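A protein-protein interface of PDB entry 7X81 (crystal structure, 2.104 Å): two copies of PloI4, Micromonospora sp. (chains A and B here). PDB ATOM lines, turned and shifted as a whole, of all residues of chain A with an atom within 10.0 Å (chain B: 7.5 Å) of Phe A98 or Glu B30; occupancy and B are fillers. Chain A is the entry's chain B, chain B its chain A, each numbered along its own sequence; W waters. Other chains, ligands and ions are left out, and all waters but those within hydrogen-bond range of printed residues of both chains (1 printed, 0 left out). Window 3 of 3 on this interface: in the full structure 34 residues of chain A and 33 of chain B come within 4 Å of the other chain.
The backbone carbonyl oxygen (O) of Val A73 lies within hydrogen-bond range of the backbone NH (N) of Met A97. The side-chain sulfur (SD) of Met A97 is in hydrogen-bond range of the side-chain amide nitrogen (NE2) of Gln A75 (3.6 Å).
Ile B36 touches Ile A65 (CG2 to CD1, 3.9 Å). O of Ile A65 touches C of Leu B38, 3.8 Å away. CD1 of Leu B38 touches CB of Ala A67, 3.9 Å away. Ala B31 touches Val A73 (CB to CG2, 3.8 Å). Val A73 touches Leu B38 (CG1 to CD2, 3.96 Å). Leu B34 touches Met A97 (CD1 to CE, 3.8 Å). Glu B30 touches Phe A98 (CB to CE1, 3.7 Å). Phe A98 touches Ala B31 (CE2 to CB, 3.8 Å). Leu B34 touches Phe A98 (CD1 to CZ, 3.7 Å).
Of chain B, only Glu B30 (3.7 Å), Ala B31 (3.8 Å) and Leu B34 (3.7 Å) come within 4 Å of Phe A98. Glu B30 touches just one residue of chain A: Phe A98. Gly B29 touches none of the printed residues of chain A. Ala B31 touches two residues of chain A. No residue of chain A comes within 4 Å of Ala B32. Printed residues of chain B within 4 Å of Ile A65: Ile B36 (3.9 Å) and Leu B38 (3.8 Å). Printed residues of chain B within 4 Å of Ala A67: Leu B38 (3.9 Å). Phe A66 touches none of the printed residues of chain B. The nearest residue of chain B that does not touch Phe A98 is Ile B36 (5.1 Å). The nearest residue of chain A that does not touch Glu B30 is Pro A99 (4.9 Å). The nearest printed residue of chain A that does not touch Ile B36 is Met A97 (4.3 Å).
Hydrophobic or aromatic side chains of chain A within 4 Å of the printed part of chain B: Ile A65, Ala A67, Val A73, Met A97 and Phe A98. Of the 11 printed residues of chain B, 5 touch a printed residue of chain A. Printed residues of chain B that touch a printed residue of chain A: Glu B30, Ala B31, Leu B34, Ile B36 and Leu B38. Hydrophobic or aromatic side chains of chain B that line the printed part of chain A: Ala B31, Leu B34, Ile B36 and Leu B38. Among the printed residues, no Asp or Glu carboxylate lies within 4 Å of a Lys or Arg side-chain nitrogen of the other chain.
No position is printed for both chains. Of the 9 pairs that touch across the chains among the printed residues, none has its exchanged pair printed and touching as well.
Water W1 lies within hydrogen-bond range of N of Thr A100 (3.0 Å) and OE2 of Glu B30 (3.3 Å).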
ATOM      1  N   ILE A  65     -22.186   9.034   4.515  1.00  0.00           N
ATOM      2  CA  ILE A  65     -22.116  10.492   4.594  1.00  0.00           C
ATOM      3  C   ILE A  65     -23.512  11.091   4.605  1.00  0.00           C
ATOM      4  O   ILE A  65     -24.409  10.638   3.882  1.00  0.00           O
ATOM      5  CB  ILE A  65     -21.291  11.050   3.425  1.00  0.00           C
ATOM      6  CG1 ILE A  65     -19.861  10.491   3.449  1.00  0.00           C
ATOM      7  CG2 ILE A  65     -21.223  12.548   3.498  1.00  0.00           C
ATOM      8  CD1 ILE A  65     -18.956  10.991   2.323  1.00  0.00           C
ATOM      9  N   PHE A  66     -23.696  12.120   5.427  1.00  0.00           N
ATOM     10  CA  PHE A  66     -24.956  12.859   5.474  1.00  0.00           C
ATOM     11  C   PHE A  66     -24.682  14.263   6.009  1.00  0.00           C
ATOM     12  O   PHE A  66     -23.529  14.667   6.217  1.00  0.00           O
ATOM     13  CB  PHE A  66     -26.013  12.110   6.308  1.00  0.00           C
ATOM     14  CG  PHE A  66     -25.809  12.189   7.810  1.00  0.00           C
ATOM     15  CD1 PHE A  66     -24.805  11.466   8.426  1.00  0.00           C
ATOM     16  CD2 PHE A  66     -26.648  12.969   8.611  1.00  0.00           C
ATOM     17  CE1 PHE A  66     -24.618  11.525   9.803  1.00  0.00           C
ATOM     18  CE2 PHE A  66     -26.465  13.035  10.009  1.00  0.00           C
ATOM     19  CZ  PHE A  66     -25.450  12.299  10.601  1.00  0.00           C
ATOM     20  N   ALA A  67     -25.749  15.023   6.223  1.00  0.00           N
ATOM     21  CA  ALA A  67     -25.575  16.373   6.734  1.00  0.00           C
ATOM     22  C   ALA A  67     -26.680  16.687   7.728  1.00  0.00           C
ATOM     23  O   ALA A  67     -27.822  16.232   7.590  1.00  0.00           O
ATOM     24  CB  ALA A  67     -25.566  17.415   5.624  1.00  0.00           C
ATOM     25  N   GLY A  71     -25.995  22.248   7.973  1.00  0.00           N
ATOM     26  CA  GLY A  71     -25.150  21.996   6.824  1.00  0.00           C
ATOM     27  C   GLY A  71     -23.850  21.298   7.120  1.00  0.00           C
ATOM     28  O   GLY A  71     -23.132  20.956   6.178  1.00  0.00           O
ATOM     29  N   THR A  72     -23.528  21.085   8.392  1.00  0.00           N
ATOM     30  CA  THR A  72     -22.333  20.329   8.747  1.00  0.00           C
ATOM     31  C   THR A  72     -22.395  18.930   8.156  1.00  0.00           C
ATOM     32  O   THR A  72     -23.327  18.165   8.426  1.00  0.00           O
ATOM     33  CB  THR A  72     -22.188  20.240  10.262  1.00  0.00           C
ATOM     34  OG1 THR A  72     -22.125  21.564  10.828  1.00  0.00           O
ATOM     35  CG2 THR A  72     -20.947  19.460  10.631  1.00  0.00           C
ATOM     36  N   VAL A  73     -21.397  18.595   7.366  1.00  0.00           N
ATOM     37  CA  VAL A  73     -21.316  17.285   6.734  1.00  0.00           C
ATOM     38  C   VAL A  73     -20.780  16.303   7.759  1.00  0.00           C
ATOM     39  O   VAL A  73     -19.766  16.557   8.429  1.00  0.00           O
ATOM     40  CB  VAL A  73     -20.434  17.338   5.477  1.00  0.00           C
ATOM     41  CG1 VAL A  73     -20.309  15.961   4.887  1.00  0.00           C
ATOM     42  CG2 VAL A  73     -21.062  18.310   4.473  1.00  0.00           C
ATOM     43  N   MET A  74     -21.465  15.188   7.906  1.00  0.00           N
ATOM     44  CA  MET A  74     -21.147  14.221   8.914  1.00  0.00           C
ATOM     45  C   MET A  74     -20.931  12.858   8.272  1.00  0.00           C
ATOM     46  O   MET A  74     -21.253  12.615   7.114  1.00  0.00           O
ATOM     47  CB  MET A  74     -22.276  14.110   9.964  1.00  0.00           C
ATOM     48  CG  MET A  74     -22.753  15.354  10.674  1.00  0.00           C
ATOM     49  SD  MET A  74     -21.746  16.048  11.783  1.00  0.00           S
ATOM     50  CE  MET A  74     -21.457  14.931  13.094  1.00  0.00           C
ATOM     51  N   GLN A  75     -20.392  11.926   9.053  1.00  0.00           N
ATOM     52  CA  GLN A  75     -20.429  10.509   8.725  1.00  0.00           C
ATOM     53  C   GLN A  75     -21.069   9.775   9.893  1.00  0.00           C
ATOM     54  O   GLN A  75     -20.902  10.152  11.063  1.00  0.00           O
ATOM     55  CB  GLN A  75     -19.023   9.966   8.423  1.00  0.00           C
ATOM     56  CG  GLN A  75     -18.417  10.575   7.164  1.00  0.00           C
ATOM     57  CD  GLN A  75     -17.085   9.951   6.730  1.00  0.00           C
ATOM     58  OE1 GLN A  75     -16.553   9.075   7.383  1.00  0.00           O
ATOM     59  NE2 GLN A  75     -16.550  10.428   5.608  1.00  0.00           N
ATOM     60  N   TYR A  95     -20.015  11.412  13.448  1.00  0.00           N
ATOM     61  CA  TYR A  95     -18.906  12.347  13.694  1.00  0.00           C
ATOM     62  C   TYR A  95     -18.771  13.319  12.522  1.00  0.00           C
ATOM     63  O   TYR A  95     -19.252  13.047  11.430  1.00  0.00           O
ATOM     64  CB  TYR A  95     -17.573  11.608  13.874  1.00  0.00           C
ATOM     65  CG  TYR A  95     -17.315  10.599  12.784  1.00  0.00           C
ATOM     66  CD1 TYR A  95     -17.828   9.327  12.864  1.00  0.00           C
ATOM     67  CD2 TYR A  95     -16.616  10.951  11.649  1.00  0.00           C
ATOM     68  CE1 TYR A  95     -17.629   8.429  11.887  1.00  0.00           C
ATOM     69  CE2 TYR A  95     -16.401  10.054  10.653  1.00  0.00           C
ATOM     70  CZ  TYR A  95     -16.907   8.783  10.775  1.00  0.00           C
ATOM     71  OH  TYR A  95     -16.712   7.857   9.782  1.00  0.00           O
ATOM     72  N   THR A  96     -18.152  14.477  12.760  1.00  0.00           N
ATOM     73  CA  THR A  96     -17.964  15.440  11.681  1.00  0.00           C
ATOM     74  C   THR A  96     -16.997  14.899  10.625  1.00  0.00           C
ATOM     75  O   THR A  96     -15.978  14.275  10.939  1.00  0.00           O
ATOM     76  CB  THR A  96     -17.423  16.752  12.226  1.00  0.00           C
ATOM     77  OG1 THR A  96     -16.159  16.504  12.876  1.00  0.00           O
ATOM     78  CG2 THR A  96     -18.385  17.348  13.225  1.00  0.00           C
ATOM     79  N   MET A  97     -17.324  15.119   9.359  1.00  0.00           N
ATOM     80  CA  MET A  97     -16.407  14.711   8.305  1.00  0.00           C
ATOM     81  C   MET A  97     -15.172  15.608   8.263  1.00  0.00           C
ATOM     82  O   MET A  97     -14.055  15.135   8.040  1.00  0.00           O
ATOM     83  CB  MET A  97     -17.096  14.748   6.936  1.00  0.00           C
ATOM     84  CG  MET A  97     -16.156  14.307   5.800  1.00  0.00           C
ATOM     85  SD  MET A  97     -17.083  13.729   4.352  1.00  0.00           S
ATOM     86  CE  MET A  97     -15.732  13.445   3.208  1.00  0.00           C
ATOM     87  N   PHE A  98     -15.353  16.889   8.417  1.00  0.00           N
ATOM     88  CA  PHE A  98     -14.235  17.793   8.194  1.00  0.00           C
ATOM     89  C   PHE A  98     -13.790  18.427   9.495  1.00  0.00           C
ATOM     90  O   PHE A  98     -14.625  18.877  10.291  1.00  0.00           O
ATOM     91  CB  PHE A  98     -14.624  18.877   7.178  1.00  0.00           C
ATOM     92  CG  PHE A  98     -14.887  18.307   5.812  1.00  0.00           C
ATOM     93  CD1 PHE A  98     -13.818  17.954   4.977  1.00  0.00           C
ATOM     94  CD2 PHE A  98     -16.194  18.053   5.382  1.00  0.00           C
ATOM     95  CE1 PHE A  98     -14.051  17.375   3.727  1.00  0.00           C
ATOM     96  CE2 PHE A  98     -16.435  17.494   4.126  1.00  0.00           C
ATOM     97  CZ  PHE A  98     -15.364  17.150   3.296  1.00  0.00           C
ATOM     98  N   PRO A  99     -12.472  18.491   9.735  1.00  0.00           N
ATOM     99  CA  PRO A  99     -11.388  18.066   8.822  1.00  0.00           C
ATOM    100  C   PRO A  99     -11.174  16.552   8.781  1.00  0.00           C
ATOM    101  O   PRO A  99     -11.459  15.834   9.750  1.00  0.00           O
ATOM    102  CB  PRO A  99     -10.158  18.794   9.397  1.00  0.00           C
ATOM    103  CG  PRO A  99     -10.467  18.929  10.854  1.00  0.00           C
ATOM    104  CD  PRO A  99     -11.951  19.084  10.986  1.00  0.00           C
ATOM    105  N   THR A 100     -10.686  16.056   7.655  1.00  0.00           N
ATOM    106  CA  THR A 100     -10.623  14.606   7.498  1.00  0.00           C
ATOM    107  C   THR A 100      -9.426  13.974   8.198  1.00  0.00           C
ATOM    108  O   THR A 100      -9.375  12.739   8.303  1.00  0.00           O
ATOM    109  CB  THR A 100     -10.589  14.239   6.017  1.00  0.00           C
ATOM    110  OG1 THR A 100      -9.470  14.858   5.388  1.00  0.00           O
ATOM    111  CG2 THR A 100     -11.830  14.722   5.320  1.00  0.00           C
ATOM    112  N   ASP A 101      -8.492  14.779   8.711  1.00  0.00           N
ATOM    113  CA  ASP A 101      -7.236  14.275   9.247  1.00  0.00           C
ATOM    114  C   ASP A 101      -7.127  14.368  10.763  1.00  0.00           C
ATOM    115  O   ASP A 101      -6.087  13.979  11.316  1.00  0.00           O
ATOM    116  CB  ASP A 101      -6.061  15.019   8.587  1.00  0.00           C
ATOM    117  CG  ASP A 101      -5.974  16.500   8.991  1.00  0.00           C
ATOM    118  OD1 ASP A 101      -6.989  17.111   9.376  1.00  0.00           O
ATOM    119  OD2 ASP A 101      -4.870  17.073   8.905  1.00  0.00           O
ATOM    120  N   GLU A 102      -8.170  14.859  11.447  1.00  0.00           N
ATOM    121  CA  GLU A 102      -8.218  14.946  12.904  1.00  0.00           C
ATOM    122  C   GLU A 102      -8.788  13.665  13.487  1.00  0.00           C
ATOM    123  O   GLU A 102      -9.533  12.950  12.818  1.00  0.00           O
ATOM    124  CB  GLU A 102      -9.071  16.144  13.342  1.00  0.00           C
ATOM    125  CG  GLU A 102     -10.571  15.916  13.160  1.00  0.00           C
ATOM    126  CD  GLU A 102     -11.490  16.971  13.804  1.00  0.00           C
ATOM    127  OE1 GLU A 102     -12.727  16.743  13.794  1.00  0.00           O
ATOM    128  OE2 GLU A 102     -10.995  18.001  14.299  1.00  0.00           O
ATOM    129  N   PRO A 103      -8.500  13.376  14.756  1.00  0.00           N
ATOM    130  CA  PRO A 103      -9.116  12.215  15.404  1.00  0.00           C
ATOM    131  C   PRO A 103     -10.617  12.378  15.548  1.00  0.00           C
ATOM    132  O   PRO A 103     -11.118  13.455  15.865  1.00  0.00           O
ATOM    133  CB  PRO A 103      -8.454  12.167  16.787  1.00  0.00           C
ATOM    134  CG  PRO A 103      -7.307  13.170  16.740  1.00  0.00           C
ATOM    135  CD  PRO A 103      -7.671  14.167  15.688  1.00  0.00           C
ATOM    136  N   LYS A 104     -11.327  11.289  15.332  1.00  0.00           N
ATOM    137  CA  LYS A 104     -12.772  11.215  15.477  1.00  0.00           C
ATOM    138  C   LYS A 104     -13.051  10.135  16.510  1.00  0.00           C
ATOM    139  O   LYS A 104     -12.233   9.236  16.724  1.00  0.00           O
ATOM    140  CB  LYS A 104     -13.457  10.875  14.145  1.00  0.00           C
ATOM    141  CG  LYS A 104     -12.966  11.667  12.943  1.00  0.00           C
ATOM    142  CD  LYS A 104     -13.417  13.148  12.990  1.00  0.00           C
ATOM    143  CE  LYS A 104     -13.023  13.854  11.713  1.00  0.00           C
ATOM    144  NZ  LYS A 104     -13.494  15.256  11.634  1.00  0.00           N
ATOM    145  N   PRO B  26     -23.372  17.968  -2.330  1.00  0.00           N
ATOM    146  CA  PRO B  26     -23.067  19.097  -1.442  1.00  0.00           C
ATOM    147  C   PRO B  26     -22.949  20.396  -2.227  1.00  0.00           C
ATOM    148  O   PRO B  26     -22.488  20.420  -3.372  1.00  0.00           O
ATOM    149  CB  PRO B  26     -21.740  18.701  -0.788  1.00  0.00           C
ATOM    150  CG  PRO B  26     -21.220  17.550  -1.593  1.00  0.00           C
ATOM    151  CD  PRO B  26     -22.402  16.868  -2.206  1.00  0.00           C
ATOM    152  N   SER B  28     -21.503  23.503  -1.153  1.00  0.00           N
ATOM    153  CA  SER B  28     -20.463  24.481  -0.864  1.00  0.00           C
ATOM    154  C   SER B  28     -19.435  23.839   0.054  1.00  0.00           C
ATOM    155  O   SER B  28     -19.483  22.636   0.317  1.00  0.00           O
ATOM    156  CB  SER B  28     -21.080  25.737  -0.240  1.00  0.00           C
ATOM    157  OG  SER B  28     -21.889  25.376   0.881  1.00  0.00           O
ATOM    158  N   GLY B  29     -18.489  24.637   0.524  1.00  0.00           N
ATOM    159  CA  GLY B  29     -17.545  24.153   1.493  1.00  0.00           C
ATOM    160  C   GLY B  29     -16.580  23.137   0.908  1.00  0.00           C
ATOM    161  O   GLY B  29     -16.419  22.986  -0.307  1.00  0.00           O
ATOM    162  N   GLU B  30     -15.896  22.450   1.822  1.00  0.00           N
ATOM    163  CA  GLU B  30     -14.963  21.411   1.407  1.00  0.00           C
ATOM    164  C   GLU B  30     -15.691  20.297   0.669  1.00  0.00           C
ATOM    165  O   GLU B  30     -15.207  19.778  -0.345  1.00  0.00           O
ATOM    166  CB  GLU B  30     -14.232  20.864   2.633  1.00  0.00           C
ATOM    167  CG  GLU B  30     -13.334  21.887   3.327  1.00  0.00           C
ATOM    168  CD  GLU B  30     -12.325  21.237   4.257  1.00  0.00           C
ATOM    169  OE1 GLU B  30     -12.421  21.484   5.483  1.00  0.00           O
ATOM    170  OE2 GLU B  30     -11.449  20.480   3.766  1.00  0.00           O
ATOM    171  N   ALA B  31     -16.883  19.946   1.142  1.00  0.00           N
ATOM    172  CA  ALA B  31     -17.579  18.797   0.594  1.00  0.00           C
ATOM    173  C   ALA B  31     -17.904  18.969  -0.880  1.00  0.00           C
ATOM    174  O   ALA B  31     -17.948  17.974  -1.612  1.00  0.00           O
ATOM    175  CB  ALA B  31     -18.858  18.536   1.401  1.00  0.00           C
ATOM    176  N   ALA B  32     -18.146  20.203  -1.344  1.00  0.00           N
ATOM    177  CA  ALA B  32     -18.460  20.394  -2.750  1.00  0.00           C
ATOM    178  C   ALA B  32     -17.276  20.075  -3.646  1.00  0.00           C
ATOM    179  O   ALA B  32     -17.478  19.769  -4.820  1.00  0.00           O
ATOM    180  CB  ALA B  32     -18.914  21.829  -3.017  1.00  0.00           C
ATOM    181  N   GLU B  33     -16.058  20.139  -3.119  1.00  0.00           N
ATOM    182  CA  GLU B  33     -14.903  19.771  -3.916  1.00  0.00           C
ATOM    183  C   GLU B  33     -14.799  18.260  -4.113  1.00  0.00           C
ATOM    184  O   GLU B  33     -13.998  17.823  -4.941  1.00  0.00           O
ATOM    185  CB  GLU B  33     -13.616  20.307  -3.280  1.00  0.00           C
ATOM    186  CG  GLU B  33     -13.387  21.824  -3.443  1.00  0.00           C
ATOM    187  CD  GLU B  33     -14.020  22.410  -4.704  1.00  0.00           C
ATOM    188  OE1 GLU B  33     -13.408  22.289  -5.788  1.00  0.00           O
ATOM    189  OE2 GLU B  33     -15.131  22.983  -4.610  1.00  0.00           O
ATOM    190  N   LEU B  34     -15.577  17.458  -3.387  1.00  0.00           N
ATOM    191  CA  LEU B  34     -15.479  16.011  -3.545  1.00  0.00           C
ATOM    192  C   LEU B  34     -16.678  15.459  -4.313  1.00  0.00           C
ATOM    193  O   LEU B  34     -17.767  16.036  -4.309  1.00  0.00           O
ATOM    194  CB  LEU B  34     -15.385  15.290  -2.187  1.00  0.00           C
ATOM    195  CG  LEU B  34     -14.369  15.916  -1.230  1.00  0.00           C
ATOM    196  CD1 LEU B  34     -14.492  15.361   0.176  1.00  0.00           C
ATOM    197  CD2 LEU B  34     -12.905  15.743  -1.731  1.00  0.00           C
ATOM    198  N   PRO B  35     -16.516  14.368  -4.975  1.00  0.00           N
ATOM    199  CA  PRO B  35     -17.625  13.754  -5.697  1.00  0.00           C
ATOM    200  C   PRO B  35     -18.495  12.857  -4.827  1.00  0.00           C
ATOM    201  O   PRO B  35     -18.824  11.727  -5.176  1.00  0.00           O
ATOM    202  CB  PRO B  35     -16.894  12.944  -6.800  1.00  0.00           C
ATOM    203  CG  PRO B  35     -15.589  12.547  -6.128  1.00  0.00           C
ATOM    204  CD  PRO B  35     -15.223  13.687  -5.204  1.00  0.00           C
ATOM    205  N   ILE B  36     -18.901  13.390  -3.674  1.00  0.00           N
ATOM    206  CA  ILE B  36     -19.678  12.624  -2.708  1.00  0.00           C
ATOM    207  C   ILE B  36     -21.160  12.985  -2.798  1.00  0.00           C
ATOM    208  O   ILE B  36     -21.553  13.953  -3.437  1.00  0.00           O
ATOM    209  CB  ILE B  36     -19.172  12.849  -1.280  1.00  0.00           C
ATOM    210  CG1 ILE B  36     -19.161  14.357  -0.936  1.00  0.00           C
ATOM    211  CG2 ILE B  36     -17.746  12.311  -1.104  1.00  0.00           C
ATOM    212  CD1 ILE B  36     -18.778  14.672   0.502  1.00  0.00           C
ATOM    213  N   LEU B  38     -24.571  13.397  -0.016  1.00  0.00           N
ATOM    214  CA  LEU B  38     -25.174  13.359   1.306  1.00  0.00           C
ATOM    215  C   LEU B  38     -26.387  12.462   1.232  1.00  0.00           C
ATOM    216  O   LEU B  38     -27.303  12.748   0.473  1.00  0.00           O
ATOM    217  CB  LEU B  38     -25.574  14.758   1.756  1.00  0.00           C
ATOM    218  CG  LEU B  38     -24.513  15.827   1.475  1.00  0.00           C
ATOM    219  CD1 LEU B  38     -25.087  17.202   1.757  1.00  0.00           C
ATOM    220  CD2 LEU B  38     -23.295  15.604   2.304  1.00  0.00           C
HETATM  221  O   HOH W   1     -10.000  18.095   5.536  1.00  0.00           O
